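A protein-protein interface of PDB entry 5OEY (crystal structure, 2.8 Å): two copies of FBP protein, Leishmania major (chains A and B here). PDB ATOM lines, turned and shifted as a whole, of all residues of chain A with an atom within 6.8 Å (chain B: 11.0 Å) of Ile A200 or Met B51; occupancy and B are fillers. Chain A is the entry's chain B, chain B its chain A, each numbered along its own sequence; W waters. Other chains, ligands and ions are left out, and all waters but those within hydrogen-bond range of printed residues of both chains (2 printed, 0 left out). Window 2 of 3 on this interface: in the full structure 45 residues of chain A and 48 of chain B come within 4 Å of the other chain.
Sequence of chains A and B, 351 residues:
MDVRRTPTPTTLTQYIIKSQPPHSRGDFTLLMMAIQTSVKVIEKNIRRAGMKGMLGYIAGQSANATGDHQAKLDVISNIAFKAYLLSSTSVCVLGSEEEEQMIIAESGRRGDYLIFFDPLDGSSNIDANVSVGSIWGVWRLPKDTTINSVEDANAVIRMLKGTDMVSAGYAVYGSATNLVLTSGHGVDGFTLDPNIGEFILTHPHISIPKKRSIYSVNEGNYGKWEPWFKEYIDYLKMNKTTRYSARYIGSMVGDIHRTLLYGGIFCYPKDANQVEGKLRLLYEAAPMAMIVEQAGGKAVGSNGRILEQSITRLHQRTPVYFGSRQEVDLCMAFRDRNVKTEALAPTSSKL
The backbone carbonyl oxygen of Lys B44 sits at hydrogen-bond distance from the guanidinium group of Arg B48, 2.9 Å away. The backbone carbonyl oxygen of Gly A189 is in hydrogen-bond range of the backbone NH of Thr A202. N of Gly A189 lies within hydrogen-bond range of O of His A203 (2.8 Å). The backbone NH (N) of Thr A191 lies within hydrogen-bond range of the backbone carbonyl oxygen (O) of Ile A200 (2.8 Å). The backbone carbonyl oxygen (O) of Glu A198 lies within hydrogen-bond range of the backbone NH (N) of Asp A193 (2.9 Å). OG1 of Thr A202 is in hydrogen-bond range of ND1 of His A203 (2.8 Å).
SD of Met B51 touches CG2 of Thr A191 (3.8 Å). Met B51 touches Asp A193. NH2 of Arg B48 touches CG of Pro A194, 3.6 Å away. Ile A200 touches Met B51 (CG2 to CG, 3.9 Å). Thr A202 touches Gly B50. Thr A202 touches Met B51 (CG2 to CG, 3.9 Å). Leu B55 touches His A203 (CD1 to NE2, 3.9 Å).
Ile A200 touches one residue of chain B. Of chain A, only Thr A191, Asp A193, Ile A200 and Thr A202 come within 4 Å of Met B51. No residue of chain B comes within 4 Å of Pro A9. No residue of chain B comes within 4 Å of Thr A10. No residue of chain B comes within 4 Å of Thr A11. No residue of chain B comes within 4 Å of Phe A190. Thr A191 touches just one residue of chain B: Met B51 (3.8 Å). Of chain B, only Met B51 (3.8 Å) comes within 4 Å of Asp A193. No residue of chain B comes within 4 Å of Leu A201. Of the printed residues of chain A, Gly B50 touches Thr A202. Printed residues of chain A within 4 Å of Arg B48: Pro A194 (3.6 Å). Printed residues of chain A within 4 Å of Leu B55: His A203 (3.9 Å). Printed residues of chain B within 4 Å of Pro A194: Arg B48 (3.6 Å). Ala B49 touches none of the printed residues of chain A. Leu A179 touches none of the printed residues of chain B. The nearest residue of chain B that does not touch Ile A200 is Gly B50 (6.9 Å). The nearest printed residue of chain B that does not touch Pro A194 is Arg B47 (4.2 Å).
Of the 19 printed residues of chain B, 4 touch a printed residue of chain A. Hydrophobic or aromatic side chains of chain B within 4 Å of the printed part of chain A: Met B51 and Leu B55. Hydrophobic or aromatic side chains of chain A within 4 Å of the printed part of chain B: Pro A194, Ile A200 and His A203. Among the printed residues, 7 pairs touch across the chains. Among the printed residues, no Asp or Glu carboxylate lies within 4 Å of a Lys or Arg side-chain nitrogen of the other chain.
No position is printed for both chains.
Water W1 lies within hydrogen-bond range of the backbone carbonyl oxygen of Leu A192 (2.7 Å) and the backbone carbonyl oxygen of Arg B47 (2.9 Å). Water W2 bridges a ring nitrogen (NE2) of His A203 (2.7 Å) and the backbone carbonyl oxygen (O) of Asp B127 (2.9 Å).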
ATOM      1  N   PRO A   9      -9.232 -16.164 -36.735  1.00  0.00           N
ATOM      2  CA  PRO A   9      -9.919 -16.812 -35.583  1.00  0.00           C
ATOM      3  C   PRO A   9     -11.087 -15.964 -35.046  1.00  0.00           C
ATOM      4  O   PRO A   9     -11.196 -14.781 -35.424  1.00  0.00           O
ATOM      5  CB  PRO A   9      -8.805 -16.912 -34.546  1.00  0.00           C
ATOM      6  CG  PRO A   9      -7.968 -15.690 -34.815  1.00  0.00           C
ATOM      7  CD  PRO A   9      -7.975 -15.513 -36.306  1.00  0.00           C
ATOM      8  N   THR A  10     -11.924 -16.563 -34.180  1.00  0.00           N
ATOM      9  CA  THR A  10     -13.072 -15.870 -33.583  1.00  0.00           C
ATOM     10  C   THR A  10     -12.675 -14.944 -32.433  1.00  0.00           C
ATOM     11  O   THR A  10     -12.262 -15.426 -31.366  1.00  0.00           O
ATOM     12  CB  THR A  10     -14.107 -16.859 -33.029  1.00  0.00           C
ATOM     13  OG1 THR A  10     -14.531 -17.713 -34.075  1.00  0.00           O
ATOM     14  CG2 THR A  10     -15.352 -16.134 -32.440  1.00  0.00           C
ATOM     15  N   THR A  11     -12.838 -13.630 -32.632  1.00  0.00           N
ATOM     16  CA  THR A  11     -12.523 -12.641 -31.594  1.00  0.00           C
ATOM     17  C   THR A  11     -13.664 -12.469 -30.583  1.00  0.00           C
ATOM     18  O   THR A  11     -14.813 -12.804 -30.864  1.00  0.00           O
ATOM     19  CB  THR A  11     -12.170 -11.257 -32.169  1.00  0.00           C
ATOM     20  OG1 THR A  11     -13.333 -10.626 -32.722  1.00  0.00           O
ATOM     21  CG2 THR A  11     -11.080 -11.353 -33.232  1.00  0.00           C
ATOM     22  N   LEU A  12     -13.324 -11.958 -29.403  1.00  0.00           N
ATOM     23  CA  LEU A  12     -14.309 -11.603 -28.397  1.00  0.00           C
ATOM     24  C   LEU A  12     -15.326 -10.598 -28.967  1.00  0.00           C
ATOM     25  O   LEU A  12     -16.526 -10.713 -28.753  1.00  0.00           O
ATOM     26  CB  LEU A  12     -13.610 -11.035 -27.153  1.00  0.00           C
ATOM     27  CG  LEU A  12     -14.496 -10.431 -26.031  1.00  0.00           C
ATOM     28  CD1 LEU A  12     -15.543 -11.422 -25.572  1.00  0.00           C
ATOM     29  CD2 LEU A  12     -13.668  -9.979 -24.832  1.00  0.00           C
ATOM     30  N   GLN A  36     -11.709  -4.627 -22.946  1.00  0.00           N
ATOM     31  CA  GLN A  36     -10.573  -5.281 -23.648  1.00  0.00           C
ATOM     32  C   GLN A  36      -9.321  -4.412 -23.706  1.00  0.00           C
ATOM     33  O   GLN A  36      -8.229  -4.876 -23.418  1.00  0.00           O
ATOM     34  CB  GLN A  36     -10.951  -5.683 -25.059  1.00  0.00           C
ATOM     35  CG  GLN A  36     -11.737  -6.978 -25.131  1.00  0.00           C
ATOM     36  CD  GLN A  36     -12.197  -7.307 -26.537  1.00  0.00           C
ATOM     37  OE1 GLN A  36     -11.500  -8.032 -27.260  1.00  0.00           O
ATOM     38  NE2 GLN A  36     -13.345  -6.739 -26.954  1.00  0.00           N
ATOM     39  N   LEU A 179      -9.593 -13.950 -20.463  1.00  0.00           N
ATOM     40  CA  LEU A 179     -10.739 -13.076 -20.213  1.00  0.00           C
ATOM     41  C   LEU A 179     -11.944 -13.950 -20.254  1.00  0.00           C
ATOM     42  O   LEU A 179     -12.277 -14.504 -21.307  1.00  0.00           O
ATOM     43  CB  LEU A 179     -10.846 -11.964 -21.251  1.00  0.00           C
ATOM     44  CG  LEU A 179     -11.771 -10.783 -20.924  1.00  0.00           C
ATOM     45  CD1 LEU A 179     -11.394  -9.615 -21.806  1.00  0.00           C
ATOM     46  CD2 LEU A 179     -13.248 -11.088 -21.129  1.00  0.00           C
ATOM     47  N   GLY A 189     -14.743 -18.398 -22.254  1.00  0.00           N
ATOM     48  CA  GLY A 189     -13.372 -18.008 -21.946  1.00  0.00           C
ATOM     49  C   GLY A 189     -12.561 -17.692 -23.183  1.00  0.00           C
ATOM     50  O   GLY A 189     -12.608 -18.412 -24.173  1.00  0.00           O
ATOM     51  N   PHE A 190     -11.822 -16.598 -23.107  1.00  0.00           N
ATOM     52  CA  PHE A 190     -11.042 -16.129 -24.201  1.00  0.00           C
ATOM     53  C   PHE A 190      -9.579 -16.037 -23.784  1.00  0.00           C
ATOM     54  O   PHE A 190      -9.283 -15.996 -22.588  1.00  0.00           O
ATOM     55  CB  PHE A 190     -11.565 -14.773 -24.645  1.00  0.00           C
ATOM     56  CG  PHE A 190     -12.952 -14.828 -25.186  1.00  0.00           C
ATOM     57  CD1 PHE A 190     -14.046 -14.935 -24.330  1.00  0.00           C
ATOM     58  CD2 PHE A 190     -13.178 -14.803 -26.559  1.00  0.00           C
ATOM     59  CE1 PHE A 190     -15.352 -15.011 -24.825  1.00  0.00           C
ATOM     60  CE2 PHE A 190     -14.476 -14.879 -27.054  1.00  0.00           C
ATOM     61  CZ  PHE A 190     -15.567 -14.973 -26.189  1.00  0.00           C
ATOM     62  N   THR A 191      -8.675 -16.019 -24.775  1.00  0.00           N
ATOM     63  CA  THR A 191      -7.238 -15.907 -24.540  1.00  0.00           C
ATOM     64  C   THR A 191      -6.656 -14.825 -25.460  1.00  0.00           C
ATOM     65  O   THR A 191      -6.924 -14.799 -26.652  1.00  0.00           O
ATOM     66  CB  THR A 191      -6.506 -17.247 -24.765  1.00  0.00           C
ATOM     67  OG1 THR A 191      -7.029 -18.257 -23.888  1.00  0.00           O
ATOM     68  CG2 THR A 191      -5.016 -17.117 -24.475  1.00  0.00           C
ATOM     69  N   LEU A 192      -5.853 -13.931 -24.887  1.00  0.00           N
ATOM     70  CA  LEU A 192      -5.233 -12.850 -25.643  1.00  0.00           C
ATOM     71  C   LEU A 192      -4.214 -13.435 -26.634  1.00  0.00           C
ATOM     72  O   LEU A 192      -3.352 -14.197 -26.253  1.00  0.00           O
ATOM     73  CB  LEU A 192      -4.543 -11.864 -24.700  1.00  0.00           C
ATOM     74  CG  LEU A 192      -3.825 -10.654 -25.278  1.00  0.00           C
ATOM     75  CD1 LEU A 192      -4.764  -9.807 -26.128  1.00  0.00           C
ATOM     76  CD2 LEU A 192      -3.214  -9.827 -24.162  1.00  0.00           C
ATOM     77  N   ASP A 193      -4.374 -13.103 -27.911  1.00  0.00           N
ATOM     78  CA  ASP A 193      -3.329 -13.307 -28.897  1.00  0.00           C
ATOM     79  C   ASP A 193      -2.462 -12.074 -28.941  1.00  0.00           C
ATOM     80  O   ASP A 193      -2.870 -11.065 -29.523  1.00  0.00           O
ATOM     81  CB  ASP A 193      -3.908 -13.528 -30.290  1.00  0.00           C
ATOM     82  CG  ASP A 193      -2.833 -13.940 -31.315  1.00  0.00           C
ATOM     83  OD1 ASP A 193      -1.615 -13.688 -31.090  1.00  0.00           O
ATOM     84  OD2 ASP A 193      -3.231 -14.572 -32.309  1.00  0.00           O
ATOM     85  N   PRO A 194      -1.260 -12.130 -28.330  1.00  0.00           N
ATOM     86  CA  PRO A 194      -0.463 -10.897 -28.263  1.00  0.00           C
ATOM     87  C   PRO A 194      -0.023 -10.369 -29.632  1.00  0.00           C
ATOM     88  O   PRO A 194       0.208  -9.174 -29.784  1.00  0.00           O
ATOM     89  CB  PRO A 194       0.718 -11.302 -27.398  1.00  0.00           C
ATOM     90  CG  PRO A 194       0.847 -12.756 -27.606  1.00  0.00           C
ATOM     91  CD  PRO A 194      -0.540 -13.276 -27.750  1.00  0.00           C
ATOM     92  N   ILE A 196      -1.854  -9.958 -32.291  1.00  0.00           N
ATOM     93  CA  ILE A 196      -2.881  -9.118 -32.900  1.00  0.00           C
ATOM     94  C   ILE A 196      -3.698  -8.338 -31.915  1.00  0.00           C
ATOM     95  O   ILE A 196      -4.589  -7.598 -32.322  1.00  0.00           O
ATOM     96  CB  ILE A 196      -3.818  -9.929 -33.815  1.00  0.00           C
ATOM     97  CG1 ILE A 196      -4.542 -11.047 -33.056  1.00  0.00           C
ATOM     98  CG2 ILE A 196      -3.018 -10.513 -34.968  1.00  0.00           C
ATOM     99  CD1 ILE A 196      -5.666 -11.682 -33.842  1.00  0.00           C
ATOM    100  N   GLU A 198      -6.057  -9.177 -29.842  1.00  0.00           N
ATOM    101  CA  GLU A 198      -7.446  -9.548 -29.785  1.00  0.00           C
ATOM    102  C   GLU A 198      -7.561 -10.750 -28.893  1.00  0.00           C
ATOM    103  O   GLU A 198      -6.630 -11.550 -28.760  1.00  0.00           O
ATOM    104  CB  GLU A 198      -7.988  -9.927 -31.158  1.00  0.00           C
ATOM    105  CG  GLU A 198      -7.951  -8.824 -32.196  1.00  0.00           C
ATOM    106  CD  GLU A 198      -8.936  -7.670 -31.980  1.00  0.00           C
ATOM    107  OE1 GLU A 198      -9.791  -7.712 -31.081  1.00  0.00           O
ATOM    108  OE2 GLU A 198      -8.862  -6.715 -32.764  1.00  0.00           O
ATOM    109  N   PHE A 199      -8.722 -10.859 -28.270  1.00  0.00           N
ATOM    110  CA  PHE A 199      -9.039 -11.985 -27.413  1.00  0.00           C
ATOM    111  C   PHE A 199      -9.727 -13.000 -28.265  1.00  0.00           C
ATOM    112  O   PHE A 199     -10.700 -12.685 -28.927  1.00  0.00           O
ATOM    113  CB  PHE A 199      -9.919 -11.534 -26.252  1.00  0.00           C
ATOM    114  CG  PHE A 199      -9.152 -10.817 -25.182  1.00  0.00           C
ATOM    115  CD1 PHE A 199      -8.528 -11.528 -24.160  1.00  0.00           C
ATOM    116  CD2 PHE A 199      -9.010  -9.431 -25.220  1.00  0.00           C
ATOM    117  CE1 PHE A 199      -7.804 -10.879 -23.193  1.00  0.00           C
ATOM    118  CE2 PHE A 199      -8.271  -8.770 -24.249  1.00  0.00           C
ATOM    119  CZ  PHE A 199      -7.659  -9.503 -23.243  1.00  0.00           C
ATOM    120  N   ILE A 200      -9.202 -14.208 -28.251  1.00  0.00           N
ATOM    121  CA  ILE A 200      -9.665 -15.282 -29.099  1.00  0.00           C
ATOM    122  C   ILE A 200     -10.431 -16.265 -28.247  1.00  0.00           C
ATOM    123  O   ILE A 200      -9.958 -16.646 -27.188  1.00  0.00           O
ATOM    124  CB  ILE A 200      -8.455 -16.013 -29.754  1.00  0.00           C
ATOM    125  CG1 ILE A 200      -7.562 -15.025 -30.530  1.00  0.00           C
ATOM    126  CG2 ILE A 200      -8.911 -17.142 -30.655  1.00  0.00           C
ATOM    127  CD1 ILE A 200      -8.281 -14.164 -31.550  1.00  0.00           C
ATOM    128  N   LEU A 201     -11.600 -16.703 -28.720  1.00  0.00           N
ATOM    129  CA  LEU A 201     -12.368 -17.766 -28.038  1.00  0.00           C
ATOM    130  C   LEU A 201     -11.551 -19.069 -27.963  1.00  0.00           C
ATOM    131  O   LEU A 201     -11.242 -19.659 -28.991  1.00  0.00           O
ATOM    132  CB  LEU A 201     -13.679 -18.034 -28.768  1.00  0.00           C
ATOM    133  CG  LEU A 201     -14.612 -19.111 -28.222  1.00  0.00           C
ATOM    134  CD1 LEU A 201     -15.094 -18.741 -26.842  1.00  0.00           C
ATOM    135  CD2 LEU A 201     -15.802 -19.273 -29.140  1.00  0.00           C
ATOM    136  N   THR A 202     -11.232 -19.498 -26.744  1.00  0.00           N
ATOM    137  CA  THR A 202     -10.511 -20.737 -26.501  1.00  0.00           C
ATOM    138  C   THR A 202     -11.240 -21.717 -25.598  1.00  0.00           C
ATOM    139  O   THR A 202     -11.013 -22.919 -25.697  1.00  0.00           O
ATOM    140  CB  THR A 202      -9.131 -20.461 -25.867  1.00  0.00           C
ATOM    141  OG1 THR A 202      -9.287 -19.639 -24.701  1.00  0.00           O
ATOM    142  CG2 THR A 202      -8.198 -19.780 -26.874  1.00  0.00           C
ATOM    143  N   HIS A 203     -12.062 -21.227 -24.685  1.00  0.00           N
ATOM    144  CA  HIS A 203     -12.752 -22.077 -23.699  1.00  0.00           C
ATOM    145  C   HIS A 203     -14.266 -21.799 -23.764  1.00  0.00           C
ATOM    146  O   HIS A 203     -14.816 -21.112 -22.886  1.00  0.00           O
ATOM    147  CB  HIS A 203     -12.229 -21.796 -22.276  1.00  0.00           C
ATOM    148  CG  HIS A 203     -10.795 -22.138 -22.074  1.00  0.00           C
ATOM    149  ND1 HIS A 203      -9.771 -21.397 -22.630  1.00  0.00           N
ATOM    150  CD2 HIS A 203     -10.209 -23.106 -21.340  1.00  0.00           C
ATOM    151  CE1 HIS A 203      -8.615 -21.928 -22.285  1.00  0.00           C
ATOM    152  NE2 HIS A 203      -8.852 -22.966 -21.500  1.00  0.00           N
ATOM    153  N   GLU B  43       8.142 -20.234 -23.303  1.00  0.00           N
ATOM    154  CA  GLU B  43       7.265 -19.103 -22.989  1.00  0.00           C
ATOM    155  C   GLU B  43       6.302 -18.771 -24.155  1.00  0.00           C
ATOM    156  O   GLU B  43       5.110 -18.565 -23.940  1.00  0.00           O
ATOM    157  CB  GLU B  43       8.101 -17.876 -22.650  1.00  0.00           C
ATOM    158  CG  GLU B  43       7.328 -16.734 -22.005  1.00  0.00           C
ATOM    159  CD  GLU B  43       6.443 -15.910 -22.959  1.00  0.00           C
ATOM    160  OE1 GLU B  43       6.895 -15.579 -24.097  1.00  0.00           O
ATOM    161  OE2 GLU B  43       5.298 -15.559 -22.527  1.00  0.00           O
ATOM    162  N   LYS B  44       6.857 -18.716 -25.363  1.00  0.00           N
ATOM    163  CA  LYS B  44       6.101 -18.475 -26.582  1.00  0.00           C
ATOM    164  C   LYS B  44       4.949 -19.435 -26.708  1.00  0.00           C
ATOM    165  O   LYS B  44       3.813 -19.041 -26.906  1.00  0.00           O
ATOM    166  CB  LYS B  44       7.028 -18.607 -27.798  1.00  0.00           C
ATOM    167  CG  LYS B  44       6.360 -18.349 -29.130  1.00  0.00           C
ATOM    168  CD  LYS B  44       6.051 -19.593 -30.006  1.00  0.00           C
ATOM    169  CE  LYS B  44       7.217 -20.569 -30.250  1.00  0.00           C
ATOM    170  NZ  LYS B  44       6.886 -21.847 -30.975  1.00  0.00           N
ATOM    171  N   ASN B  45       5.262 -20.711 -26.563  1.00  0.00           N
ATOM    172  CA  ASN B  45       4.276 -21.790 -26.642  1.00  0.00           C
ATOM    173  C   ASN B  45       3.211 -21.734 -25.562  1.00  0.00           C
ATOM    174  O   ASN B  45       2.062 -21.967 -25.820  1.00  0.00           O
ATOM    175  CB  ASN B  45       4.996 -23.128 -26.605  1.00  0.00           C
ATOM    176  CG  ASN B  45       5.680 -23.434 -27.929  1.00  0.00           C
ATOM    177  OD1 ASN B  45       5.013 -23.657 -28.923  1.00  0.00           O
ATOM    178  ND2 ASN B  45       6.988 -23.501 -27.935  1.00  0.00           N
ATOM    179  N   ILE B  46       3.604 -21.418 -24.337  1.00  0.00           N
ATOM    180  CA  ILE B  46       2.649 -21.374 -23.222  1.00  0.00           C
ATOM    181  C   ILE B  46       1.659 -20.233 -23.443  1.00  0.00           C
ATOM    182  O   ILE B  46       0.472 -20.423 -23.258  1.00  0.00           O
ATOM    183  CB  ILE B  46       3.345 -21.262 -21.845  1.00  0.00           C
ATOM    184  CG1 ILE B  46       4.155 -22.520 -21.555  1.00  0.00           C
ATOM    185  CG2 ILE B  46       2.324 -21.101 -20.724  1.00  0.00           C
ATOM    186  CD1 ILE B  46       5.227 -22.295 -20.519  1.00  0.00           C
ATOM    187  N   ARG B  47       2.147 -19.066 -23.848  1.00  0.00           N
ATOM    188  CA  ARG B  47       1.296 -17.876 -23.987  1.00  0.00           C
ATOM    189  C   ARG B  47       0.149 -18.082 -24.995  1.00  0.00           C
ATOM    190  O   ARG B  47      -0.940 -17.531 -24.815  1.00  0.00           O
ATOM    191  CB  ARG B  47       2.158 -16.629 -24.317  1.00  0.00           C
ATOM    192  CG  ARG B  47       1.466 -15.264 -24.201  1.00  0.00           C
ATOM    193  CD  ARG B  47       2.464 -14.083 -23.987  1.00  0.00           C
ATOM    194  NE  ARG B  47       3.181 -14.049 -22.705  1.00  0.00           N
ATOM    195  CZ  ARG B  47       2.662 -13.638 -21.538  1.00  0.00           C
ATOM    196  NH1 ARG B  47       1.373 -13.264 -21.444  1.00  0.00           N
ATOM    197  NH2 ARG B  47       3.430 -13.626 -20.454  1.00  0.00           N
ATOM    198  N   ARG B  48       0.394 -18.898 -26.020  1.00  0.00           N
ATOM    199  CA  ARG B  48      -0.572 -19.144 -27.088  1.00  0.00           C
ATOM    200  C   ARG B  48      -1.110 -20.579 -27.123  1.00  0.00           C
ATOM    201  O   ARG B  48      -1.903 -20.923 -28.009  1.00  0.00           O
ATOM    202  CB  ARG B  48       0.074 -18.843 -28.437  1.00  0.00           C
ATOM    203  CG  ARG B  48       0.417 -17.390 -28.702  1.00  0.00           C
ATOM    204  CD  ARG B  48       1.383 -17.281 -29.871  1.00  0.00           C
ATOM    205  NE  ARG B  48       2.062 -15.986 -29.895  1.00  0.00           N
ATOM    206  CZ  ARG B  48       3.086 -15.614 -29.105  1.00  0.00           C
ATOM    207  NH1 ARG B  48       3.612 -16.425 -28.177  1.00  0.00           N
ATOM    208  NH2 ARG B  48       3.589 -14.383 -29.233  1.00  0.00           N
ATOM    209  N   ALA B  49      -0.743 -21.400 -26.142  1.00  0.00           N
ATOM    210  CA  ALA B  49      -1.181 -22.806 -26.090  1.00  0.00           C
ATOM    211  C   ALA B  49      -2.660 -23.032 -26.378  1.00  0.00           C
ATOM    212  O   ALA B  49      -3.015 -23.976 -27.074  1.00  0.00           O
ATOM    213  CB  ALA B  49      -0.817 -23.423 -24.741  1.00  0.00           C
ATOM    214  N   GLY B  50      -3.514 -22.184 -25.822  1.00  0.00           N
ATOM    215  CA  GLY B  50      -4.959 -22.298 -26.028  1.00  0.00           C
ATOM    216  C   GLY B  50      -5.419 -22.255 -27.480  1.00  0.00           C
ATOM    217  O   GLY B  50      -6.349 -22.956 -27.852  1.00  0.00           O
ATOM    218  N   MET B  51      -4.797 -21.396 -28.277  1.00  0.00           N
ATOM    219  CA  MET B  51      -5.160 -21.228 -29.679  1.00  0.00           C
ATOM    220  C   MET B  51      -4.461 -22.211 -30.596  1.00  0.00           C
ATOM    221  O   MET B  51      -4.978 -22.505 -31.673  1.00  0.00           O
ATOM    222  CB  MET B  51      -4.811 -19.819 -30.162  1.00  0.00           C
ATOM    223  CG  MET B  51      -5.569 -18.686 -29.469  1.00  0.00           C
ATOM    224  SD  MET B  51      -4.663 -17.823 -28.174  1.00  0.00           S
ATOM    225  CE  MET B  51      -3.243 -17.140 -29.032  1.00  0.00           C
ATOM    226  N   LYS B  52      -3.294 -22.696 -30.184  1.00  0.00           N
ATOM    227  CA  LYS B  52      -2.525 -23.697 -30.950  1.00  0.00           C
ATOM    228  C   LYS B  52      -2.843 -25.166 -30.554  1.00  0.00           C
ATOM    229  O   LYS B  52      -2.127 -26.084 -30.939  1.00  0.00           O
ATOM    230  CB  LYS B  52      -1.016 -23.413 -30.825  1.00  0.00           C
ATOM    231  CG  LYS B  52      -0.487 -22.390 -31.820  1.00  0.00           C
ATOM    232  CD  LYS B  52       1.043 -22.269 -31.789  1.00  0.00           C
ATOM    233  CE  LYS B  52       1.549 -21.491 -30.575  1.00  0.00           C
ATOM    234  NZ  LYS B  52       3.038 -21.362 -30.511  1.00  0.00           N
ATOM    235  N   GLY B  53      -3.928 -25.385 -29.810  1.00  0.00           N
ATOM    236  CA  GLY B  53      -4.351 -26.728 -29.425  1.00  0.00           C
ATOM    237  C   GLY B  53      -3.430 -27.512 -28.496  1.00  0.00           C
ATOM    238  O   GLY B  53      -3.601 -28.719 -28.363  1.00  0.00           O
ATOM    239  N   MET B  54      -2.541 -26.832 -27.769  1.00  0.00           N
ATOM    240  CA  MET B  54      -1.579 -27.500 -26.884  1.00  0.00           C
ATOM    241  C   MET B  54      -1.933 -27.470 -25.396  1.00  0.00           C
ATOM    242  O   MET B  54      -1.092 -27.612 -24.528  1.00  0.00           O
ATOM    243  CB  MET B  54      -0.233 -26.867 -27.044  1.00  0.00           C
ATOM    244  CG  MET B  54       0.216 -26.847 -28.479  1.00  0.00           C
ATOM    245  SD  MET B  54       1.859 -26.112 -28.618  1.00  0.00           S
ATOM    246  CE  MET B  54       1.573 -24.377 -28.318  1.00  0.00           C
ATOM    247  N   LEU B  55      -3.213 -27.399 -25.098  1.00  0.00           N
ATOM    248  CA  LEU B  55      -3.656 -27.458 -23.741  1.00  0.00           C
ATOM    249  C   LEU B  55      -3.987 -28.945 -23.554  1.00  0.00           C
ATOM    250  O   LEU B  55      -4.174 -29.693 -24.528  1.00  0.00           O
ATOM    251  CB  LEU B  55      -4.764 -26.401 -23.514  1.00  0.00           C
ATOM    252  CG  LEU B  55      -4.214 -24.996 -23.198  1.00  0.00           C
ATOM    253  CD1 LEU B  55      -5.363 -24.122 -22.699  1.00  0.00           C
ATOM    254  CD2 LEU B  55      -3.086 -25.017 -22.166  1.00  0.00           C
ATOM    255  N   GLY B  56      -3.938 -29.386 -22.302  1.00  0.00           N
ATOM    256  CA  GLY B  56      -4.128 -30.797 -21.965  1.00  0.00           C
ATOM    257  C   GLY B  56      -2.929 -31.707 -22.140  1.00  0.00           C
ATOM    258  O   GLY B  56      -1.802 -31.315 -21.837  1.00  0.00           O
ATOM    259  N   LYS B  72       1.090 -32.029 -23.282  1.00  0.00           N
ATOM    260  CA  LYS B  72       1.744 -31.754 -24.588  1.00  0.00           C
ATOM    261  C   LYS B  72       2.934 -30.777 -24.488  1.00  0.00           C
ATOM    262  O   LYS B  72       3.932 -30.851 -25.254  1.00  0.00           O
ATOM    263  CB  LYS B  72       0.746 -31.210 -25.600  1.00  0.00           C
ATOM    264  CG  LYS B  72      -0.454 -32.103 -25.859  1.00  0.00           C
ATOM    265  CD  LYS B  72      -1.490 -31.412 -26.709  1.00  0.00           C
ATOM    266  CE  LYS B  72      -2.801 -32.115 -26.515  1.00  0.00           C
ATOM    267  NZ  LYS B  72      -3.737 -31.740 -27.596  1.00  0.00           N
ATOM    268  N   LEU B  73       2.816 -29.849 -23.543  1.00  0.00           N
ATOM    269  CA  LEU B  73       3.877 -28.867 -23.293  1.00  0.00           C
ATOM    270  C   LEU B  73       5.086 -29.443 -22.577  1.00  0.00           C
ATOM    271  O   LEU B  73       6.152 -28.896 -22.727  1.00  0.00           O
ATOM    272  CB  LEU B  73       3.344 -27.640 -22.570  1.00  0.00           C
ATOM    273  CG  LEU B  73       2.423 -26.773 -23.431  1.00  0.00           C
ATOM    274  CD1 LEU B  73       1.751 -25.740 -22.566  1.00  0.00           C
ATOM    275  CD2 LEU B  73       3.170 -26.078 -24.551  1.00  0.00           C
ATOM    276  N   ILE B 126      -1.382 -25.890 -16.272  1.00  0.00           N
ATOM    277  CA  ILE B 126      -1.367 -25.008 -17.434  1.00  0.00           C
ATOM    278  C   ILE B 126      -2.754 -24.740 -17.915  1.00  0.00           C
ATOM    279  O   ILE B 126      -3.108 -23.595 -18.200  1.00  0.00           O
ATOM    280  CB  ILE B 126      -0.600 -25.585 -18.614  1.00  0.00           C
ATOM    281  CG1 ILE B 126       0.727 -26.108 -18.140  1.00  0.00           C
ATOM    282  CG2 ILE B 126      -0.430 -24.523 -19.696  1.00  0.00           C
ATOM    283  CD1 ILE B 126       1.268 -27.187 -19.019  1.00  0.00           C
ATOM    284  N   ASP B 127      -3.548 -25.796 -17.989  1.00  0.00           N
ATOM    285  CA  ASP B 127      -4.950 -25.654 -18.338  1.00  0.00           C
ATOM    286  C   ASP B 127      -5.715 -24.624 -17.525  1.00  0.00           C
ATOM    287  O   ASP B 127      -6.691 -24.088 -18.032  1.00  0.00           O
ATOM    288  CB  ASP B 127      -5.687 -26.982 -18.247  1.00  0.00           C
ATOM    289  CG  ASP B 127      -5.097 -28.045 -19.144  1.00  0.00           C
ATOM    290  OD1 ASP B 127      -4.039 -27.804 -19.770  1.00  0.00           O
ATOM    291  OD2 ASP B 127      -5.688 -29.141 -19.223  1.00  0.00           O
ATOM    292  N   ASN B 129      -4.133 -21.843 -16.203  1.00  0.00           N
ATOM    293  CA  ASN B 129      -3.283 -20.650 -16.224  1.00  0.00           C
ATOM    294  C   ASN B 129      -2.624 -20.303 -14.890  1.00  0.00           C
ATOM    295  O   ASN B 129      -2.449 -19.130 -14.557  1.00  0.00           O
ATOM    296  CB  ASN B 129      -4.072 -19.450 -16.730  1.00  0.00           C
ATOM    297  CG  ASN B 129      -3.193 -18.389 -17.355  1.00  0.00           C
ATOM    298  OD1 ASN B 129      -1.999 -18.579 -17.602  1.00  0.00           O
ATOM    299  ND2 ASN B 129      -3.791 -17.240 -17.604  1.00  0.00           N
HETATM  300  O   HOH W   1      -2.226 -15.095 -23.937  1.00  0.00           O
HETATM  301  O   HOH W   2      -7.749 -25.236 -20.423  1.00  0.00           O
